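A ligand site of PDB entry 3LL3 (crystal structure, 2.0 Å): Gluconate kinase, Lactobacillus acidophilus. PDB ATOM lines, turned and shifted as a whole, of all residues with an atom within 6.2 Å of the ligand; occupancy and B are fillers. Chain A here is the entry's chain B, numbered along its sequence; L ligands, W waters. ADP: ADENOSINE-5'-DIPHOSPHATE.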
ATOM      1  N   ASN A 258      -2.487  25.786  14.470  1.00  0.00           N
ATOM      2  CA  ASN A 258      -1.784  26.669  15.371  1.00  0.00           C
ATOM      3  C   ASN A 258      -2.544  26.764  16.673  1.00  0.00           C
ATOM      4  O   ASN A 258      -3.742  27.003  16.678  1.00  0.00           O
ATOM      5  CB  ASN A 258      -1.634  28.067  14.781  1.00  0.00           C
ATOM      6  CG  ASN A 258      -0.828  28.969  15.690  1.00  0.00           C
ATOM      7  OD1 ASN A 258       0.373  28.815  15.834  1.00  0.00           O
ATOM      8  ND2 ASN A 258      -1.516  29.907  16.334  1.00  0.00           N
ATOM      9  N   VAL A 259      -1.866  26.563  17.793  1.00  0.00           N
ATOM     10  CA  VAL A 259      -2.520  26.788  19.069  1.00  0.00           C
ATOM     11  C   VAL A 259      -1.649  27.596  20.012  1.00  0.00           C
ATOM     12  O   VAL A 259      -0.686  27.082  20.585  1.00  0.00           O
ATOM     13  CB  VAL A 259      -2.993  25.496  19.759  1.00  0.00           C
ATOM     14  CG1 VAL A 259      -3.938  25.860  20.900  1.00  0.00           C
ATOM     15  CG2 VAL A 259      -3.675  24.563  18.765  1.00  0.00           C
ATOM     16  N   GLY A 260      -1.998  28.859  20.175  1.00  0.00           N
ATOM     17  CA  GLY A 260      -1.384  29.696  21.190  1.00  0.00           C
ATOM     18  C   GLY A 260      -2.380  29.949  22.311  1.00  0.00           C
ATOM     19  O   GLY A 260      -2.912  29.008  22.899  1.00  0.00           O
ATOM     20  N   THR A 261      -2.631  31.217  22.598  1.00  0.00           N
ATOM     21  CA  THR A 261      -3.697  31.585  23.516  1.00  0.00           C
ATOM     22  C   THR A 261      -5.031  31.052  22.970  1.00  0.00           C
ATOM     23  O   THR A 261      -5.808  30.401  23.672  1.00  0.00           O
ATOM     24  CB  THR A 261      -3.795  33.109  23.688  1.00  0.00           C
ATOM     25  OG1 THR A 261      -2.570  33.590  24.250  1.00  0.00           O
ATOM     26  CG2 THR A 261      -4.920  33.465  24.614  1.00  0.00           C
ATOM     27  N   SER A 262      -5.267  31.344  21.692  1.00  0.00           N
ATOM     28  CA  SER A 262      -6.360  30.719  20.970  1.00  0.00           C
ATOM     29  C   SER A 262      -5.787  29.849  19.852  1.00  0.00           C
ATOM     30  O   SER A 262      -4.574  29.721  19.694  1.00  0.00           O
ATOM     31  CB  SER A 262      -7.306  31.763  20.399  1.00  0.00           C
ATOM     32  OG  SER A 262      -6.645  32.550  19.441  1.00  0.00           O
ATOM     33  N   GLY A 299      -7.955  27.853  23.500  1.00  0.00           N
ATOM     34  CA  GLY A 299      -6.676  27.188  23.372  1.00  0.00           C
ATOM     35  C   GLY A 299      -5.863  27.270  24.653  1.00  0.00           C
ATOM     36  O   GLY A 299      -6.328  26.870  25.714  1.00  0.00           O
ATOM     37  N   GLY A 300      -4.655  27.805  24.567  1.00  0.00           N
ATOM     38  CA  GLY A 300      -3.801  27.984  25.723  1.00  0.00           C
ATOM     39  C   GLY A 300      -4.396  28.859  26.801  1.00  0.00           C
ATOM     40  O   GLY A 300      -4.004  28.778  27.955  1.00  0.00           O
ATOM     41  N   ILE A 301      -5.339  29.729  26.423  1.00  0.00           N
ATOM     42  CA  ILE A 301      -6.000  30.567  27.416  1.00  0.00           C
ATOM     43  C   ILE A 301      -6.721  29.695  28.462  1.00  0.00           C
ATOM     44  O   ILE A 301      -6.735  30.017  29.650  1.00  0.00           O
ATOM     45  CB  ILE A 301      -6.979  31.561  26.751  1.00  0.00           C
ATOM     46  CG1 ILE A 301      -7.522  32.555  27.777  1.00  0.00           C
ATOM     47  CG2 ILE A 301      -8.123  30.841  26.054  1.00  0.00           C
ATOM     48  CD1 ILE A 301      -8.272  33.739  27.144  1.00  0.00           C
ATOM     49  N   VAL A 302      -7.286  28.576  28.011  1.00  0.00           N
ATOM     50  CA  VAL A 302      -7.990  27.649  28.901  1.00  0.00           C
ATOM     51  C   VAL A 302      -6.986  26.836  29.716  1.00  0.00           C
ATOM     52  O   VAL A 302      -7.184  26.619  30.912  1.00  0.00           O
ATOM     53  CB  VAL A 302      -8.968  26.754  28.099  1.00  0.00           C
ATOM     54  CG1 VAL A 302      -9.578  25.658  28.998  1.00  0.00           C
ATOM     55  CG2 VAL A 302     -10.061  27.634  27.465  1.00  0.00           C
ATOM     56  N   PHE A 303      -5.877  26.441  29.101  1.00  0.00           N
ATOM     57  CA  PHE A 303      -4.785  25.809  29.824  1.00  0.00           C
ATOM     58  C   PHE A 303      -4.321  26.716  30.967  1.00  0.00           C
ATOM     59  O   PHE A 303      -4.103  26.242  32.087  1.00  0.00           O
ATOM     60  CB  PHE A 303      -3.603  25.542  28.879  1.00  0.00           C
ATOM     61  CG  PHE A 303      -2.403  24.928  29.556  1.00  0.00           C
ATOM     62  CD1 PHE A 303      -1.399  25.729  30.065  1.00  0.00           C
ATOM     63  CD2 PHE A 303      -2.304  23.556  29.704  1.00  0.00           C
ATOM     64  CE1 PHE A 303      -0.290  25.155  30.697  1.00  0.00           C
ATOM     65  CE2 PHE A 303      -1.211  22.984  30.320  1.00  0.00           C
ATOM     66  CZ  PHE A 303      -0.203  23.777  30.818  1.00  0.00           C
ATOM     67  N   ASN A 304      -4.155  27.996  30.670  1.00  0.00           N
ATOM     68  CA  ASN A 304      -3.699  28.963  31.666  1.00  0.00           C
ATOM     69  C   ASN A 304      -4.708  29.118  32.808  1.00  0.00           C
ATOM     70  O   ASN A 304      -4.347  29.157  33.966  1.00  0.00           O
ATOM     71  CB  ASN A 304      -3.375  30.319  31.016  1.00  0.00           C
ATOM     72  CG  ASN A 304      -2.726  31.284  32.002  1.00  0.00           C
ATOM     73  OD1 ASN A 304      -3.304  32.326  32.359  1.00  0.00           O
ATOM     74  ND2 ASN A 304      -1.530  30.945  32.449  1.00  0.00           N
ATOM     75  N   TRP A 305      -5.997  29.163  32.471  1.00  0.00           N
ATOM     76  CA  TRP A 305      -7.054  29.173  33.480  1.00  0.00           C
ATOM     77  C   TRP A 305      -6.921  27.979  34.430  1.00  0.00           C
ATOM     78  O   TRP A 305      -6.937  28.141  35.655  1.00  0.00           O
ATOM     79  CB  TRP A 305      -8.423  29.145  32.834  1.00  0.00           C
ATOM     80  CG  TRP A 305      -9.497  28.914  33.840  1.00  0.00           C
ATOM     81  CD1 TRP A 305     -10.038  29.838  34.677  1.00  0.00           C
ATOM     82  CD2 TRP A 305     -10.143  27.675  34.126  1.00  0.00           C
ATOM     83  NE1 TRP A 305     -10.999  29.256  35.470  1.00  0.00           N
ATOM     84  CE2 TRP A 305     -11.080  27.927  35.163  1.00  0.00           C
ATOM     85  CE3 TRP A 305     -10.044  26.378  33.614  1.00  0.00           C
ATOM     86  CZ2 TRP A 305     -11.893  26.921  35.684  1.00  0.00           C
ATOM     87  CZ3 TRP A 305     -10.841  25.389  34.135  1.00  0.00           C
ATOM     88  CH2 TRP A 305     -11.769  25.663  35.167  1.00  0.00           C
ATOM     89  N   ARG A 307      -4.338  25.914  34.889  1.00  0.00           N
ATOM     90  CA  ARG A 307      -3.080  26.017  35.616  1.00  0.00           C
ATOM     91  C   ARG A 307      -3.260  26.783  36.921  1.00  0.00           C
ATOM     92  O   ARG A 307      -2.790  26.352  37.974  1.00  0.00           O
ATOM     93  CB  ARG A 307      -2.018  26.705  34.749  1.00  0.00           C
ATOM     94  CG  ARG A 307      -0.667  26.878  35.410  1.00  0.00           C
ATOM     95  CD  ARG A 307       0.293  27.653  34.484  1.00  0.00           C
ATOM     96  NE  ARG A 307      -0.151  29.021  34.283  1.00  0.00           N
ATOM     97  CZ  ARG A 307       0.086  30.011  35.140  1.00  0.00           C
ATOM     98  NH1 ARG A 307       0.771  29.774  36.255  1.00  0.00           N
ATOM     99  NH2 ARG A 307      -0.353  31.241  34.894  1.00  0.00           N
ATOM    100  N   PRO A 317       3.637  25.987  33.895  1.00  0.00           N
ATOM    101  CA  PRO A 317       3.053  25.117  32.871  1.00  0.00           C
ATOM    102  C   PRO A 317       3.675  23.722  32.897  1.00  0.00           C
ATOM    103  O   PRO A 317       2.954  22.720  32.743  1.00  0.00           O
ATOM    104  CB  PRO A 317       3.411  25.823  31.568  1.00  0.00           C
ATOM    105  CG  PRO A 317       3.372  27.243  31.930  1.00  0.00           C
ATOM    106  CD  PRO A 317       3.971  27.309  33.333  1.00  0.00           C
ATOM    107  N   GLN A 318       4.975  23.643  33.115  1.00  0.00           N
ATOM    108  CA  GLN A 318       5.623  22.337  33.180  1.00  0.00           C
ATOM    109  C   GLN A 318       5.098  21.495  34.352  1.00  0.00           C
ATOM    110  O   GLN A 318       4.917  20.293  34.209  1.00  0.00           O
ATOM    111  CB  GLN A 318       7.147  22.435  33.202  1.00  0.00           C
ATOM    112  CG  GLN A 318       7.823  21.070  33.003  1.00  0.00           C
ATOM    113  CD  GLN A 318       7.447  20.415  31.688  1.00  0.00           C
ATOM    114  OE1 GLN A 318       7.496  21.046  30.630  1.00  0.00           O
ATOM    115  NE2 GLN A 318       7.055  19.153  31.736  1.00  0.00           N
ATOM    116  N   LEU A 321       1.818  20.054  33.351  1.00  0.00           N
ATOM    117  CA  LEU A 321       2.046  18.963  32.417  1.00  0.00           C
ATOM    118  C   LEU A 321       2.522  17.700  33.139  1.00  0.00           C
ATOM    119  O   LEU A 321       2.019  16.603  32.890  1.00  0.00           O
ATOM    120  CB  LEU A 321       3.043  19.387  31.331  1.00  0.00           C
ATOM    121  CG  LEU A 321       2.552  20.465  30.350  1.00  0.00           C
ATOM    122  CD1 LEU A 321       3.642  20.817  29.326  1.00  0.00           C
ATOM    123  CD2 LEU A 321       1.262  20.053  29.652  1.00  0.00           C
ATOM    124  N   GLY A 401       2.678  26.998  17.864  1.00  0.00           N
ATOM    125  CA  GLY A 401       1.960  27.638  18.954  1.00  0.00           C
ATOM    126  C   GLY A 401       2.488  27.263  20.321  1.00  0.00           C
ATOM    127  O   GLY A 401       2.962  26.150  20.511  1.00  0.00           O
ATOM    128  N   GLY A 402       2.424  28.187  21.268  1.00  0.00           N
ATOM    129  CA  GLY A 402       2.943  27.964  22.600  1.00  0.00           C
ATOM    130  C   GLY A 402       2.237  26.823  23.307  1.00  0.00           C
ATOM    131  O   GLY A 402       2.836  26.143  24.144  1.00  0.00           O
ATOM    132  N   PHE A 403       0.970  26.576  22.982  1.00  0.00           N
ATOM    133  CA  PHE A 403       0.261  25.466  23.623  1.00  0.00           C
ATOM    134  C   PHE A 403       0.869  24.135  23.212  1.00  0.00           C
ATOM    135  O   PHE A 403       0.821  23.153  23.964  1.00  0.00           O
ATOM    136  CB  PHE A 403      -1.240  25.484  23.351  1.00  0.00           C
ATOM    137  CG  PHE A 403      -1.982  24.338  23.974  1.00  0.00           C
ATOM    138  CD1 PHE A 403      -2.099  24.237  25.357  1.00  0.00           C
ATOM    139  CD2 PHE A 403      -2.531  23.342  23.189  1.00  0.00           C
ATOM    140  CE1 PHE A 403      -2.779  23.177  25.938  1.00  0.00           C
ATOM    141  CE2 PHE A 403      -3.208  22.273  23.760  1.00  0.00           C
ATOM    142  CZ  PHE A 403      -3.328  22.182  25.123  1.00  0.00           C
ATOM    143  N   LEU A 404       1.471  24.113  22.015  1.00  0.00           N
ATOM    144  CA  LEU A 404       2.040  22.897  21.421  1.00  0.00           C
ATOM    145  C   LEU A 404       3.533  22.758  21.676  1.00  0.00           C
ATOM    146  O   LEU A 404       4.230  22.048  20.968  1.00  0.00           O
ATOM    147  CB  LEU A 404       1.818  22.895  19.908  1.00  0.00           C
ATOM    148  CG  LEU A 404       0.529  22.308  19.356  1.00  0.00           C
ATOM    149  CD1 LEU A 404      -0.623  22.434  20.342  1.00  0.00           C
ATOM    150  CD2 LEU A 404       0.203  22.934  18.018  1.00  0.00           C
ATOM    151  N   LYS A 405       4.017  23.446  22.705  1.00  0.00           N
ATOM    152  CA  LYS A 405       5.429  23.502  23.009  1.00  0.00           C
ATOM    153  C   LYS A 405       5.991  22.141  23.414  1.00  0.00           C
ATOM    154  O   LYS A 405       7.051  21.732  22.955  1.00  0.00           O
ATOM    155  CB  LYS A 405       5.631  24.484  24.156  1.00  0.00           C
ATOM    156  CG  LYS A 405       7.051  24.937  24.370  1.00  0.00           C
ATOM    157  CD  LYS A 405       7.193  25.707  25.702  1.00  0.00           C
ATOM    158  CE  LYS A 405       5.966  26.574  26.038  1.00  0.00           C
ATOM    159  NZ  LYS A 405       5.719  27.721  25.099  1.00  0.00           N
ATOM    160  N   SER A 406       5.278  21.449  24.294  1.00  0.00           N
ATOM    161  CA  SER A 406       5.803  20.232  24.919  1.00  0.00           C
ATOM    162  C   SER A 406       5.673  19.002  24.030  1.00  0.00           C
ATOM    163  O   SER A 406       4.700  18.861  23.277  1.00  0.00           O
ATOM    164  CB  SER A 406       5.080  19.983  26.253  1.00  0.00           C
ATOM    165  OG  SER A 406       3.780  19.487  26.010  1.00  0.00           O
ATOM    166  N   VAL A 409       2.188  17.303  24.684  1.00  0.00           N
ATOM    167  CA  VAL A 409       1.023  17.776  23.965  1.00  0.00           C
ATOM    168  C   VAL A 409       1.157  17.463  22.476  1.00  0.00           C
ATOM    169  O   VAL A 409       0.189  17.142  21.800  1.00  0.00           O
ATOM    170  CB  VAL A 409       0.801  19.278  24.209  1.00  0.00           C
ATOM    171  CG1 VAL A 409      -0.285  19.836  23.274  1.00  0.00           C
ATOM    172  CG2 VAL A 409       0.429  19.513  25.692  1.00  0.00           C
ATOM    173  N   GLN A 427       8.054  29.589  13.980  1.00  0.00           N
ATOM    174  CA  GLN A 427       6.739  29.911  14.551  1.00  0.00           C
ATOM    175  C   GLN A 427       6.097  31.147  13.901  1.00  0.00           C
ATOM    176  O   GLN A 427       4.870  31.241  13.837  1.00  0.00           O
ATOM    177  CB  GLN A 427       6.840  30.174  16.063  1.00  0.00           C
ATOM    178  CG  GLN A 427       7.448  29.058  16.877  1.00  0.00           C
ATOM    179  CD  GLN A 427       6.684  27.757  16.739  1.00  0.00           C
ATOM    180  OE1 GLN A 427       7.197  26.807  16.171  1.00  0.00           O
ATOM    181  NE2 GLN A 427       5.452  27.722  17.245  1.00  0.00           N
HETATM  182  PB  ADP L   1       0.309  34.069  21.376  1.00  0.00           P
HETATM  183  O1B ADP L   1       1.103  34.643  20.041  1.00  0.00           O
HETATM  184  O2B ADP L   1      -0.196  35.195  22.152  1.00  0.00           O
HETATM  185  O3B ADP L   1      -0.949  33.083  20.957  1.00  0.00           O
HETATM  186  PA  ADP L   1       1.895  31.707  22.228  1.00  0.00           P
HETATM  187  O1A ADP L   1       3.386  31.622  22.941  1.00  0.00           O
HETATM  188  O2A ADP L   1       1.895  31.092  20.909  1.00  0.00           O
HETATM  189  O3A ADP L   1       1.405  33.295  22.351  1.00  0.00           O
HETATM  190  O5' ADP L   1       0.792  30.810  23.123  1.00  0.00           O
HETATM  191  C5' ADP L   1       0.399  31.300  24.388  1.00  0.00           C
HETATM  192  C4' ADP L   1      -0.137  30.194  25.310  1.00  0.00           C
HETATM  193  O4' ADP L   1       0.782  29.202  25.745  1.00  0.00           O
HETATM  194  C3' ADP L   1      -0.912  30.598  26.607  1.00  0.00           C
HETATM  195  O3' ADP L   1      -2.293  30.702  26.417  1.00  0.00           O
HETATM  196  C2' ADP L   1      -0.367  29.596  27.732  1.00  0.00           C
HETATM  197  O2' ADP L   1      -1.328  29.142  28.637  1.00  0.00           O
HETATM  198  C1' ADP L   1       0.258  28.535  26.847  1.00  0.00           C
HETATM  199  N9  ADP L   1       1.395  27.839  27.429  1.00  0.00           N
HETATM  200  C8  ADP L   1       2.522  28.367  27.911  1.00  0.00           C
HETATM  201  N7  ADP L   1       3.413  27.304  28.214  1.00  0.00           N
HETATM  202  C5  ADP L   1       2.781  26.102  27.858  1.00  0.00           C
HETATM  203  C6  ADP L   1       3.195  24.744  27.936  1.00  0.00           C
HETATM  204  N6  ADP L   1       4.520  24.429  28.434  1.00  0.00           N
HETATM  205  N1  ADP L   1       2.372  23.773  27.534  1.00  0.00           N
HETATM  206  C2  ADP L   1       1.129  24.078  27.052  1.00  0.00           C
HETATM  207  N3  ADP L   1       0.718  25.407  26.979  1.00  0.00           N
HETATM  208  C4  ADP L   1       1.548  26.396  27.389  1.00  0.00           C
HETATM  209  O   HOH W   1      -0.077  28.841  31.290  1.00  0.00           O
HETATM  210  O   HOH W   2       4.334  30.745  25.308  1.00  0.00           O
HETATM  211  O   HOH W   3       6.653  22.382  28.380  1.00  0.00           O
HETATM  212  O   HOH W   4      -3.021  32.560  28.333  1.00  0.00           O
HETATM  213  O   HOH W   5       6.930  25.499  29.703  1.00  0.00           O
HETATM  214  O   HOH W   6       3.813  31.090  18.868  1.00  0.00           O
HETATM  215  O   HOH W   7       0.592  31.455  18.464  1.00  0.00           O
HETATM  216  O   HOH W   8       2.739  21.938  25.680  1.00  0.00           O
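Water W8 lies within hydrogen-bond range of N1 of the ligand (2.6 Å), OG of Ser 406 (2.7 Å) and O of Phe 403 (2.8 Å). Water W2 bridges O1A of the ligand (2.7 Å) and NZ of Lys 405 (3.3 Å). Water W7 bridges O2A of the ligand (2.8 Å) and ND2 of Asn 258 (3.4 Å). Water W1 lies within hydrogen-bond range of the side-chain amide nitrogen of Asn 304 (2.8 Å), an oxygen (O2') of the ligand (2.9 Å) and the guanidinium group of Arg 307 (3.0 Å). Water W3 bridges OE1 of Gln 318 and N6 of the ligand.
CA of Gly 260 touches O5' of the ligand, at 3.1 Å. CD1 of Phe 303 touches O2' of the ligand, 3.7 Å away. Asn 304 touches the ligand. CB of Pro 317 touches N6 of the ligand, at 3.6 Å. CD1 of Leu 321 touches N1 of the ligand, at 3.7 Å. Gly 401 touches the ligand (C to O2A, 3.9 Å). Phe 403 touches the ligand (O to C2, 3.2 Å). CE of Lys 405 touches N7 of the ligand, at 3.4 Å. The nearest printed residue that does not touch the ligand is Ser 262 (4.7 Å).
The backbone carbonyl oxygen (O) of Thr 261 is in hydrogen-bond range of the backbone NH (N) of Gly 300. The backbone NH (N) of Gly 300 lies within hydrogen-bond range of the backbone carbonyl oxygen (O) of Gly 260, at 2.7 Å. O of Gly 402 sits close to NZ of Lys 405, 3.4 Å away. The backbone NH (N) of Ile 301 lies within hydrogen-bond range of the backbone carbonyl oxygen (O) of Thr 261, at 2.9 Å. The backbone carbonyl oxygen (O) of Thr 261 lies close to the backbone NH (N) of Gly 299, 3.3 Å away. O of Val 259 sits at hydrogen-bond distance from N of Phe 403 (3.0 Å). The side-chain amide nitrogen of Asn 304 sits close to the guanidinium group of Arg 307 (2.7 Å). NE2 of Gln 427 lies close to N of Gly 401, 2.9 Å away.
O2' of the ligand lies within hydrogen-bond range of O of Gly 300, 2.8 Å away. N of Gly 402 sits at hydrogen-bond distance from O2A of the ligand (3.0 Å). N of Thr 261 is in hydrogen-bond range of O3B of the ligand (3.0 Å). The backbone NH of Ile 301 sits at hydrogen-bond distance from an oxygen (O3') of the ligand (3.2 Å).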
